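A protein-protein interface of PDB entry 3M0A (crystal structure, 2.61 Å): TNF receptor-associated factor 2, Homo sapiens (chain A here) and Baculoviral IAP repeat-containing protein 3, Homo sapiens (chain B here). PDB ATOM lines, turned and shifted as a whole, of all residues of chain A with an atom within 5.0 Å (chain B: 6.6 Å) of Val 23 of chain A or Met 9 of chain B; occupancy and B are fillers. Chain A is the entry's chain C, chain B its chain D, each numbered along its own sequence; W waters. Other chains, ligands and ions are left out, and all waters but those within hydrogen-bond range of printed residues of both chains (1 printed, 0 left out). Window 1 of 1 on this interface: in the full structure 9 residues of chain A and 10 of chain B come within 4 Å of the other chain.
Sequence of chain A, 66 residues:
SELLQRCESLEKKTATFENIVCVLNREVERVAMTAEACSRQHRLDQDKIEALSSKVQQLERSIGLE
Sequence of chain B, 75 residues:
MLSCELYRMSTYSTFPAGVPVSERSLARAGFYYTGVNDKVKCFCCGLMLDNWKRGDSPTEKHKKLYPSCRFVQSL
Printed residues of chain B that touch a printed residue of chain A: Leu 6, Met 9, Ser 10, Tyr 12, Ser 13, Glu 23 and Arg 24. Hydrophobic or aromatic side chains of chain B within 4 Å of the printed part of chain A: Met 9 and Tyr 12. Of the 9 printed residues of chain A, 7 touch a printed residue of chain B. Hydrophobic or aromatic side chains of chain A that line the printed part of chain B: Ile 20, Val 23 and Leu 24.
Water W1 bridges the backbone NH (N) of Arg 24 of chain B and the side-chain carboxylate (OE1) of Glu 27 of chain A.
O of Tyr 7 of chain B is in hydrogen-bond range of OG of Ser 10 of chain B, at 2.5 Å. The side-chain hydroxyl (OG) of Ser 13 of chain B is in hydrogen-bond range of the backbone carbonyl oxygen (O) of Ser 10 of chain B (3.5 Å). The side-chain hydroxyl of Tyr 12 of chain B lies within hydrogen-bond range of the backbone carbonyl oxygen of Phe 31 of chain B.
Printed residues of chain B within 4 Å of Cys 22 of chain A: Ser 13 (3.8 Å). Printed residues of chain B within 4 Å of Val 23 of chain A: Met 9, Tyr 12, Ser 13 and Glu 23. Of the printed residues of chain B, Glu 27 of chain A touches Arg 24. Glu 5 of chain B touches none of the printed residues of chain A. Met 9 of chain B touches just these residues of chain A: Ile 20 (3.8 Å), Val 23 (3.6 Å) and Leu 24 (3.6 Å). Of the printed residues of chain A, Ser 10 of chain B touches Asn 19 and Ile 20. Of the printed residues of chain A, Tyr 12 of chain B touches Val 23 (3.7 Å) and Arg 26 (3.1 Å). The nearest printed residue of chain B that does not touch Leu 24 of chain A is Leu 6 of chain B (6.2 Å).
OG of Ser 13 of chain B is in hydrogen-bond range of ND2 of Asn 19 of chain A. The backbone carbonyl oxygen (O) of Ser 13 of chain B lies within hydrogen-bond range of the side-chain sulfur (SG) of Cys 22 of chain A (3.8 Å). NH2 of Arg 26 of chain A is in hydrogen-bond range of O of Tyr 12 of chain B (3.1 Å). The backbone carbonyl oxygen (O) of Ser 13 of chain B lies within hydrogen-bond range of the guanidinium group (NH1) of Arg 26 of chain A (3.4 Å). The guanidinium group of Arg 26 of chain A is in salt-bridge range of the side-chain carboxylate of Glu 23 of chain B, at 3.2 Å. The side-chain carboxylate (OE2) of Glu 27 of chain A lies within salt-bridge range of the guanidinium group (NE) of Arg 24 of chain B, at 2.9 Å.
Among the printed residues, pairs that only touch across the chains: Asn 19 of chain A with Ser 10 of chain B (3.7 Å), Ile 20 of chain A with Leu 6 of chain B (3.7 Å), Ile 20 of chain A with Met 9 of chain B (3.8 Å), Ile 20 of chain A with Ser 10 of chain B (3.6 Å), Val 23 of chain A with Met 9 of chain B (3.6 Å), Val 23 of chain A with Tyr 12 of chain B (3.7 Å), Val 23 of chain A with Ser 13 of chain B (3.6 Å), Val 23 of chain A with Glu 23 of chain B (3.8 Å), Leu 24 of chain A with Met 9 of chain B (3.6 Å) and Leu 24 of chain A with Arg 24 of chain B (3.5 Å).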
ATOM      1  N   ASN A  19       0.443 -30.970   1.774  1.00  0.00           N
ATOM      2  CA  ASN A  19       0.941 -30.035   2.753  1.00  0.00           C
ATOM      3  C   ASN A  19       0.077 -29.964   3.983  1.00  0.00           C
ATOM      4  O   ASN A  19       0.633 -29.889   5.097  1.00  0.00           O
ATOM      5  CB  ASN A  19       1.181 -28.642   2.186  1.00  0.00           C
ATOM      6  CG  ASN A  19       2.444 -28.579   1.289  1.00  0.00           C
ATOM      7  OD1 ASN A  19       2.355 -28.296   0.117  1.00  0.00           O
ATOM      8  ND2 ASN A  19       3.618 -28.816   1.868  1.00  0.00           N
ATOM      9  N   ILE A  20      -1.251 -29.980   3.843  1.00  0.00           N
ATOM     10  CA  ILE A  20      -2.090 -29.819   5.038  1.00  0.00           C
ATOM     11  C   ILE A  20      -1.940 -31.018   5.930  1.00  0.00           C
ATOM     12  O   ILE A  20      -1.861 -30.878   7.159  1.00  0.00           O
ATOM     13  CB  ILE A  20      -3.576 -29.715   4.706  1.00  0.00           C
ATOM     14  CG1 ILE A  20      -3.885 -28.367   4.113  1.00  0.00           C
ATOM     15  CG2 ILE A  20      -4.461 -29.899   5.981  1.00  0.00           C
ATOM     16  CD1 ILE A  20      -5.278 -28.334   3.611  1.00  0.00           C
ATOM     17  N   VAL A  21      -1.896 -32.214   5.330  1.00  0.00           N
ATOM     18  CA  VAL A  21      -1.818 -33.474   6.119  1.00  0.00           C
ATOM     19  C   VAL A  21      -0.468 -33.631   6.837  1.00  0.00           C
ATOM     20  O   VAL A  21      -0.342 -34.278   7.919  1.00  0.00           O
ATOM     21  CB  VAL A  21      -2.115 -34.664   5.202  1.00  0.00           C
ATOM     22  CG1 VAL A  21      -1.447 -35.915   5.671  1.00  0.00           C
ATOM     23  CG2 VAL A  21      -3.655 -34.776   4.947  1.00  0.00           C
ATOM     24  N   CYS A  22       0.544 -33.025   6.244  1.00  0.00           N
ATOM     25  CA  CYS A  22       1.847 -32.944   6.887  1.00  0.00           C
ATOM     26  C   CYS A  22       1.840 -32.100   8.217  1.00  0.00           C
ATOM     27  O   CYS A  22       2.504 -32.456   9.229  1.00  0.00           O
ATOM     28  CB  CYS A  22       2.853 -32.455   5.858  1.00  0.00           C
ATOM     29  SG  CYS A  22       4.228 -31.620   6.580  1.00  0.00           S
ATOM     30  N   VAL A  23       1.036 -31.037   8.240  1.00  0.00           N
ATOM     31  CA  VAL A  23       0.779 -30.269   9.479  1.00  0.00           C
ATOM     32  C   VAL A  23      -0.038 -31.065  10.518  1.00  0.00           C
ATOM     33  O   VAL A  23       0.206 -30.978  11.749  1.00  0.00           O
ATOM     34  CB  VAL A  23       0.090 -28.919   9.203  1.00  0.00           C
ATOM     35  CG1 VAL A  23      -0.161 -28.227  10.504  1.00  0.00           C
ATOM     36  CG2 VAL A  23       0.949 -28.040   8.285  1.00  0.00           C
ATOM     37  N   LEU A  24      -1.016 -31.834  10.050  1.00  0.00           N
ATOM     38  CA  LEU A  24      -1.826 -32.572  10.996  1.00  0.00           C
ATOM     39  C   LEU A  24      -0.971 -33.675  11.599  1.00  0.00           C
ATOM     40  O   LEU A  24      -1.034 -33.905  12.812  1.00  0.00           O
ATOM     41  CB  LEU A  24      -3.042 -33.134  10.306  1.00  0.00           C
ATOM     42  CG  LEU A  24      -3.913 -31.951   9.828  1.00  0.00           C
ATOM     43  CD1 LEU A  24      -4.783 -32.389   8.716  1.00  0.00           C
ATOM     44  CD2 LEU A  24      -4.735 -31.292  10.951  1.00  0.00           C
ATOM     45  N   ASN A  25      -0.130 -34.344  10.791  1.00  0.00           N
ATOM     46  CA  ASN A  25       0.827 -35.336  11.389  1.00  0.00           C
ATOM     47  C   ASN A  25       1.582 -34.736  12.584  1.00  0.00           C
ATOM     48  O   ASN A  25       1.782 -35.400  13.602  1.00  0.00           O
ATOM     49  CB  ASN A  25       1.855 -35.789  10.352  1.00  0.00           C
ATOM     50  CG  ASN A  25       2.689 -37.037  10.803  1.00  0.00           C
ATOM     51  OD1 ASN A  25       2.697 -37.460  12.009  1.00  0.00           O
ATOM     52  ND2 ASN A  25       3.408 -37.642   9.806  1.00  0.00           N
ATOM     53  N   ARG A  26       2.055 -33.496  12.426  1.00  0.00           N
ATOM     54  CA  ARG A  26       2.821 -32.844  13.469  1.00  0.00           C
ATOM     55  C   ARG A  26       1.931 -32.549  14.633  1.00  0.00           C
ATOM     56  O   ARG A  26       2.324 -32.802  15.776  1.00  0.00           O
ATOM     57  CB  ARG A  26       3.429 -31.542  12.988  1.00  0.00           C
ATOM     58  CG  ARG A  26       4.729 -31.747  12.331  1.00  0.00           C
ATOM     59  CD  ARG A  26       5.681 -30.684  12.835  1.00  0.00           C
ATOM     60  NE  ARG A  26       5.140 -29.357  12.541  1.00  0.00           N
ATOM     61  CZ  ARG A  26       5.153 -28.779  11.325  1.00  0.00           C
ATOM     62  NH1 ARG A  26       5.703 -29.418  10.279  1.00  0.00           N
ATOM     63  NH2 ARG A  26       4.608 -27.558  11.153  1.00  0.00           N
ATOM     64  N   GLU A  27       0.731 -32.014  14.356  1.00  0.00           N
ATOM     65  CA  GLU A  27      -0.228 -31.749  15.419  1.00  0.00           C
ATOM     66  C   GLU A  27      -0.504 -33.008  16.234  1.00  0.00           C
ATOM     67  O   GLU A  27      -0.302 -32.981  17.490  1.00  0.00           O
ATOM     68  CB  GLU A  27      -1.511 -31.216  14.854  1.00  0.00           C
ATOM     69  CG  GLU A  27      -2.460 -30.806  15.918  1.00  0.00           C
ATOM     70  CD  GLU A  27      -3.568 -29.838  15.423  1.00  0.00           C
ATOM     71  OE1 GLU A  27      -3.872 -29.792  14.154  1.00  0.00           O
ATOM     72  OE2 GLU A  27      -4.131 -29.124  16.352  1.00  0.00           O
ATOM     73  N   CYS B   4     -10.640 -20.931   3.894  1.00  0.00           N
ATOM     74  CA  CYS B   4      -9.391 -20.126   3.907  1.00  0.00           C
ATOM     75  C   CYS B   4      -8.423 -20.613   4.954  1.00  0.00           C
ATOM     76  O   CYS B   4      -7.253 -20.882   4.625  1.00  0.00           O
ATOM     77  CB  CYS B   4      -9.653 -18.667   4.126  1.00  0.00           C
ATOM     78  SG  CYS B   4     -10.708 -18.013   2.850  1.00  0.00           S
ATOM     79  N   GLU B   5      -8.929 -20.782   6.185  1.00  0.00           N
ATOM     80  CA  GLU B   5      -8.137 -21.249   7.327  1.00  0.00           C
ATOM     81  C   GLU B   5      -7.239 -22.417   6.935  1.00  0.00           C
ATOM     82  O   GLU B   5      -6.006 -22.374   7.141  1.00  0.00           O
ATOM     83  CB  GLU B   5      -9.016 -21.627   8.530  1.00  0.00           C
ATOM     84  CG  GLU B   5      -8.187 -22.057   9.712  1.00  0.00           C
ATOM     85  CD  GLU B   5      -8.970 -22.381  11.004  1.00  0.00           C
ATOM     86  OE1 GLU B   5      -9.130 -23.611  11.339  1.00  0.00           O
ATOM     87  OE2 GLU B   5      -9.369 -21.397  11.692  1.00  0.00           O
ATOM     88  N   LEU B   6      -7.842 -23.449   6.345  1.00  0.00           N
ATOM     89  CA  LEU B   6      -7.051 -24.583   5.876  1.00  0.00           C
ATOM     90  C   LEU B   6      -6.072 -24.229   4.775  1.00  0.00           C
ATOM     91  O   LEU B   6      -4.992 -24.810   4.720  1.00  0.00           O
ATOM     92  CB  LEU B   6      -7.919 -25.721   5.410  1.00  0.00           C
ATOM     93  CG  LEU B   6      -8.640 -26.344   6.578  1.00  0.00           C
ATOM     94  CD1 LEU B   6      -9.639 -27.396   6.052  1.00  0.00           C
ATOM     95  CD2 LEU B   6      -7.606 -27.010   7.345  1.00  0.00           C
ATOM     96  N   TYR B   7      -6.389 -23.289   3.897  1.00  0.00           N
ATOM     97  CA  TYR B   7      -5.348 -22.911   2.950  1.00  0.00           C
ATOM     98  C   TYR B   7      -4.208 -22.280   3.707  1.00  0.00           C
ATOM     99  O   TYR B   7      -3.058 -22.644   3.470  1.00  0.00           O
ATOM    100  CB  TYR B   7      -5.837 -21.971   1.887  1.00  0.00           C
ATOM    101  CG  TYR B   7      -6.357 -22.746   0.700  1.00  0.00           C
ATOM    102  CD1 TYR B   7      -7.739 -22.984   0.542  1.00  0.00           C
ATOM    103  CD2 TYR B   7      -5.467 -23.300  -0.238  1.00  0.00           C
ATOM    104  CE1 TYR B   7      -8.217 -23.717  -0.565  1.00  0.00           C
ATOM    105  CE2 TYR B   7      -5.900 -24.024  -1.331  1.00  0.00           C
ATOM    106  CZ  TYR B   7      -7.267 -24.227  -1.518  1.00  0.00           C
ATOM    107  OH  TYR B   7      -7.681 -24.965  -2.631  1.00  0.00           O
ATOM    108  N   ARG B   8      -4.507 -21.396   4.642  1.00  0.00           N
ATOM    109  CA  ARG B   8      -3.470 -20.816   5.539  1.00  0.00           C
ATOM    110  C   ARG B   8      -2.763 -21.867   6.349  1.00  0.00           C
ATOM    111  O   ARG B   8      -1.556 -21.784   6.626  1.00  0.00           O
ATOM    112  CB  ARG B   8      -4.091 -19.803   6.519  1.00  0.00           C
ATOM    113  CG  ARG B   8      -4.291 -18.512   5.738  1.00  0.00           C
ATOM    114  CD  ARG B   8      -5.200 -17.561   6.439  1.00  0.00           C
ATOM    115  NE  ARG B   8      -5.938 -18.014   7.643  1.00  0.00           N
ATOM    116  CZ  ARG B   8      -7.241 -17.695   7.806  1.00  0.00           C
ATOM    117  NH1 ARG B   8      -7.856 -17.031   6.835  1.00  0.00           N
ATOM    118  NH2 ARG B   8      -7.949 -18.029   8.883  1.00  0.00           N
ATOM    119  N   MET B   9      -3.465 -22.932   6.683  1.00  0.00           N
ATOM    120  CA  MET B   9      -2.748 -23.909   7.454  1.00  0.00           C
ATOM    121  C   MET B   9      -1.711 -24.612   6.565  1.00  0.00           C
ATOM    122  O   MET B   9      -0.659 -25.043   7.065  1.00  0.00           O
ATOM    123  CB  MET B   9      -3.737 -24.898   8.096  1.00  0.00           C
ATOM    124  CG  MET B   9      -3.060 -25.952   8.986  1.00  0.00           C
ATOM    125  SD  MET B   9      -4.285 -26.559  10.239  1.00  0.00           S
ATOM    126  CE  MET B   9      -4.632 -28.103   9.366  1.00  0.00           C
ATOM    127  N   SER B  10      -1.986 -24.751   5.270  1.00  0.00           N
ATOM    128  CA  SER B  10      -1.090 -25.571   4.478  1.00  0.00           C
ATOM    129  C   SER B  10       0.206 -24.857   4.401  1.00  0.00           C
ATOM    130  O   SER B  10       1.263 -25.530   4.196  1.00  0.00           O
ATOM    131  CB  SER B  10      -1.578 -25.761   3.036  1.00  0.00           C
ATOM    132  OG  SER B  10      -1.769 -24.487   2.452  1.00  0.00           O
ATOM    133  N   THR B  11       0.221 -23.517   4.532  1.00  0.00           N
ATOM    134  CA  THR B  11       1.604 -22.923   4.409  1.00  0.00           C
ATOM    135  C   THR B  11       2.484 -23.286   5.606  1.00  0.00           C
ATOM    136  O   THR B  11       3.665 -22.879   5.661  1.00  0.00           O
ATOM    137  CB  THR B  11       1.605 -21.442   4.467  1.00  0.00           C
ATOM    138  OG1 THR B  11       1.051 -21.079   5.762  1.00  0.00           O
ATOM    139  CG2 THR B  11       0.761 -20.870   3.238  1.00  0.00           C
ATOM    140  N   TYR B  12       1.931 -23.947   6.636  1.00  0.00           N
ATOM    141  CA  TYR B  12       2.844 -24.302   7.761  1.00  0.00           C
ATOM    142  C   TYR B  12       3.634 -25.593   7.564  1.00  0.00           C
ATOM    143  O   TYR B  12       4.363 -25.978   8.475  1.00  0.00           O
ATOM    144  CB  TYR B  12       2.107 -24.311   9.114  1.00  0.00           C
ATOM    145  CG  TYR B  12       1.671 -22.894   9.520  1.00  0.00           C
ATOM    146  CD1 TYR B  12       2.505 -22.074  10.292  1.00  0.00           C
ATOM    147  CD2 TYR B  12       0.478 -22.351   9.059  1.00  0.00           C
ATOM    148  CE1 TYR B  12       2.155 -20.791  10.616  1.00  0.00           C
ATOM    149  CE2 TYR B  12       0.111 -21.043   9.413  1.00  0.00           C
ATOM    150  CZ  TYR B  12       0.956 -20.278  10.164  1.00  0.00           C
ATOM    151  OH  TYR B  12       0.582 -18.969  10.482  1.00  0.00           O
ATOM    152  N   SER B  13       3.524 -26.296   6.431  1.00  0.00           N
ATOM    153  CA  SER B  13       4.215 -27.613   6.328  1.00  0.00           C
ATOM    154  C   SER B  13       5.734 -27.554   6.611  1.00  0.00           C
ATOM    155  O   SER B  13       6.349 -28.532   7.020  1.00  0.00           O
ATOM    156  CB  SER B  13       4.013 -28.200   4.963  1.00  0.00           C
ATOM    157  OG  SER B  13       4.308 -27.208   3.978  1.00  0.00           O
ATOM    158  N   THR B  14       6.304 -26.373   6.419  1.00  0.00           N
ATOM    159  CA  THR B  14       7.725 -26.058   6.539  1.00  0.00           C
ATOM    160  C   THR B  14       8.004 -25.370   7.839  1.00  0.00           C
ATOM    161  O   THR B  14       9.127 -24.998   8.123  1.00  0.00           O
ATOM    162  CB  THR B  14       8.118 -24.984   5.475  1.00  0.00           C
ATOM    163  OG1 THR B  14       7.050 -24.007   5.378  1.00  0.00           O
ATOM    164  CG2 THR B  14       8.347 -25.613   4.112  1.00  0.00           C
ATOM    165  N   GLU B  23       0.515 -24.208  14.991  1.00  0.00           N
ATOM    166  CA  GLU B  23       0.205 -23.880  13.600  1.00  0.00           C
ATOM    167  C   GLU B  23      -1.294 -23.571  13.477  1.00  0.00           C
ATOM    168  O   GLU B  23      -1.683 -22.500  13.026  1.00  0.00           O
ATOM    169  CB  GLU B  23       0.577 -25.032  12.663  1.00  0.00           C
ATOM    170  CG  GLU B  23       2.086 -25.259  12.469  1.00  0.00           C
ATOM    171  CD  GLU B  23       2.625 -26.240  13.452  1.00  0.00           C
ATOM    172  OE1 GLU B  23       2.288 -27.442  13.315  1.00  0.00           O
ATOM    173  OE2 GLU B  23       3.334 -25.793  14.390  1.00  0.00           O
ATOM    174  N   ARG B  24      -2.138 -24.498  13.941  1.00  0.00           N
ATOM    175  CA  ARG B  24      -3.605 -24.326  13.946  1.00  0.00           C
ATOM    176  C   ARG B  24      -4.046 -23.000  14.540  1.00  0.00           C
ATOM    177  O   ARG B  24      -4.859 -22.305  13.942  1.00  0.00           O
ATOM    178  CB  ARG B  24      -4.280 -25.466  14.678  1.00  0.00           C
ATOM    179  CG  ARG B  24      -5.749 -25.320  14.695  1.00  0.00           C
ATOM    180  CD  ARG B  24      -6.334 -26.470  15.479  1.00  0.00           C
ATOM    181  NE  ARG B  24      -6.140 -27.741  14.788  1.00  0.00           N
ATOM    182  CZ  ARG B  24      -6.814 -28.109  13.705  1.00  0.00           C
ATOM    183  NH1 ARG B  24      -7.736 -27.321  13.204  1.00  0.00           N
ATOM    184  NH2 ARG B  24      -6.590 -29.274  13.156  1.00  0.00           N
ATOM    185  N   ALA B  27      -2.816 -19.987  11.951  1.00  0.00           N
ATOM    186  CA  ALA B  27      -3.701 -19.906  10.807  1.00  0.00           C
ATOM    187  C   ALA B  27      -5.094 -19.453  11.264  1.00  0.00           C
ATOM    188  O   ALA B  27      -5.777 -18.662  10.567  1.00  0.00           O
ATOM    189  CB  ALA B  27      -3.798 -21.214  10.131  1.00  0.00           C
ATOM    190  N   PHE B  31      -3.108 -15.787  10.125  1.00  0.00           N
ATOM    191  CA  PHE B  31      -1.708 -15.583   9.720  1.00  0.00           C
ATOM    192  C   PHE B  31      -1.269 -16.785   8.954  1.00  0.00           C
ATOM    193  O   PHE B  31      -1.560 -17.932   9.443  1.00  0.00           O
ATOM    194  CB  PHE B  31      -0.796 -15.637  10.938  1.00  0.00           C
ATOM    195  CG  PHE B  31      -0.961 -14.506  11.849  1.00  0.00           C
ATOM    196  CD1 PHE B  31      -0.515 -13.220  11.456  1.00  0.00           C
ATOM    197  CD2 PHE B  31      -1.595 -14.684  13.077  1.00  0.00           C
ATOM    198  CE1 PHE B  31      -0.672 -12.075  12.302  1.00  0.00           C
ATOM    199  CE2 PHE B  31      -1.757 -13.592  13.924  1.00  0.00           C
ATOM    200  CZ  PHE B  31      -1.271 -12.253  13.525  1.00  0.00           C
ATOM    201  N   TYR B  32      -0.536 -16.593   7.850  1.00  0.00           N
ATOM    202  CA  TYR B  32       0.035 -17.729   7.186  1.00  0.00           C
ATOM    203  C   TYR B  32       1.550 -17.638   7.246  1.00  0.00           C
ATOM    204  O   TYR B  32       2.101 -16.559   7.506  1.00  0.00           O
ATOM    205  CB  TYR B  32      -0.350 -17.695   5.734  1.00  0.00           C
ATOM    206  CG  TYR B  32       0.094 -16.475   4.943  1.00  0.00           C
ATOM    207  CD1 TYR B  32      -0.840 -15.555   4.540  1.00  0.00           C
ATOM    208  CD2 TYR B  32       1.430 -16.319   4.481  1.00  0.00           C
ATOM    209  CE1 TYR B  32      -0.499 -14.448   3.732  1.00  0.00           C
ATOM    210  CE2 TYR B  32       1.806 -15.185   3.658  1.00  0.00           C
ATOM    211  CZ  TYR B  32       0.836 -14.255   3.317  1.00  0.00           C
ATOM    212  OH  TYR B  32       1.092 -13.123   2.521  1.00  0.00           O
HETATM  213  O   HOH W   1      -1.631 -27.503  14.336  1.00  0.00           O
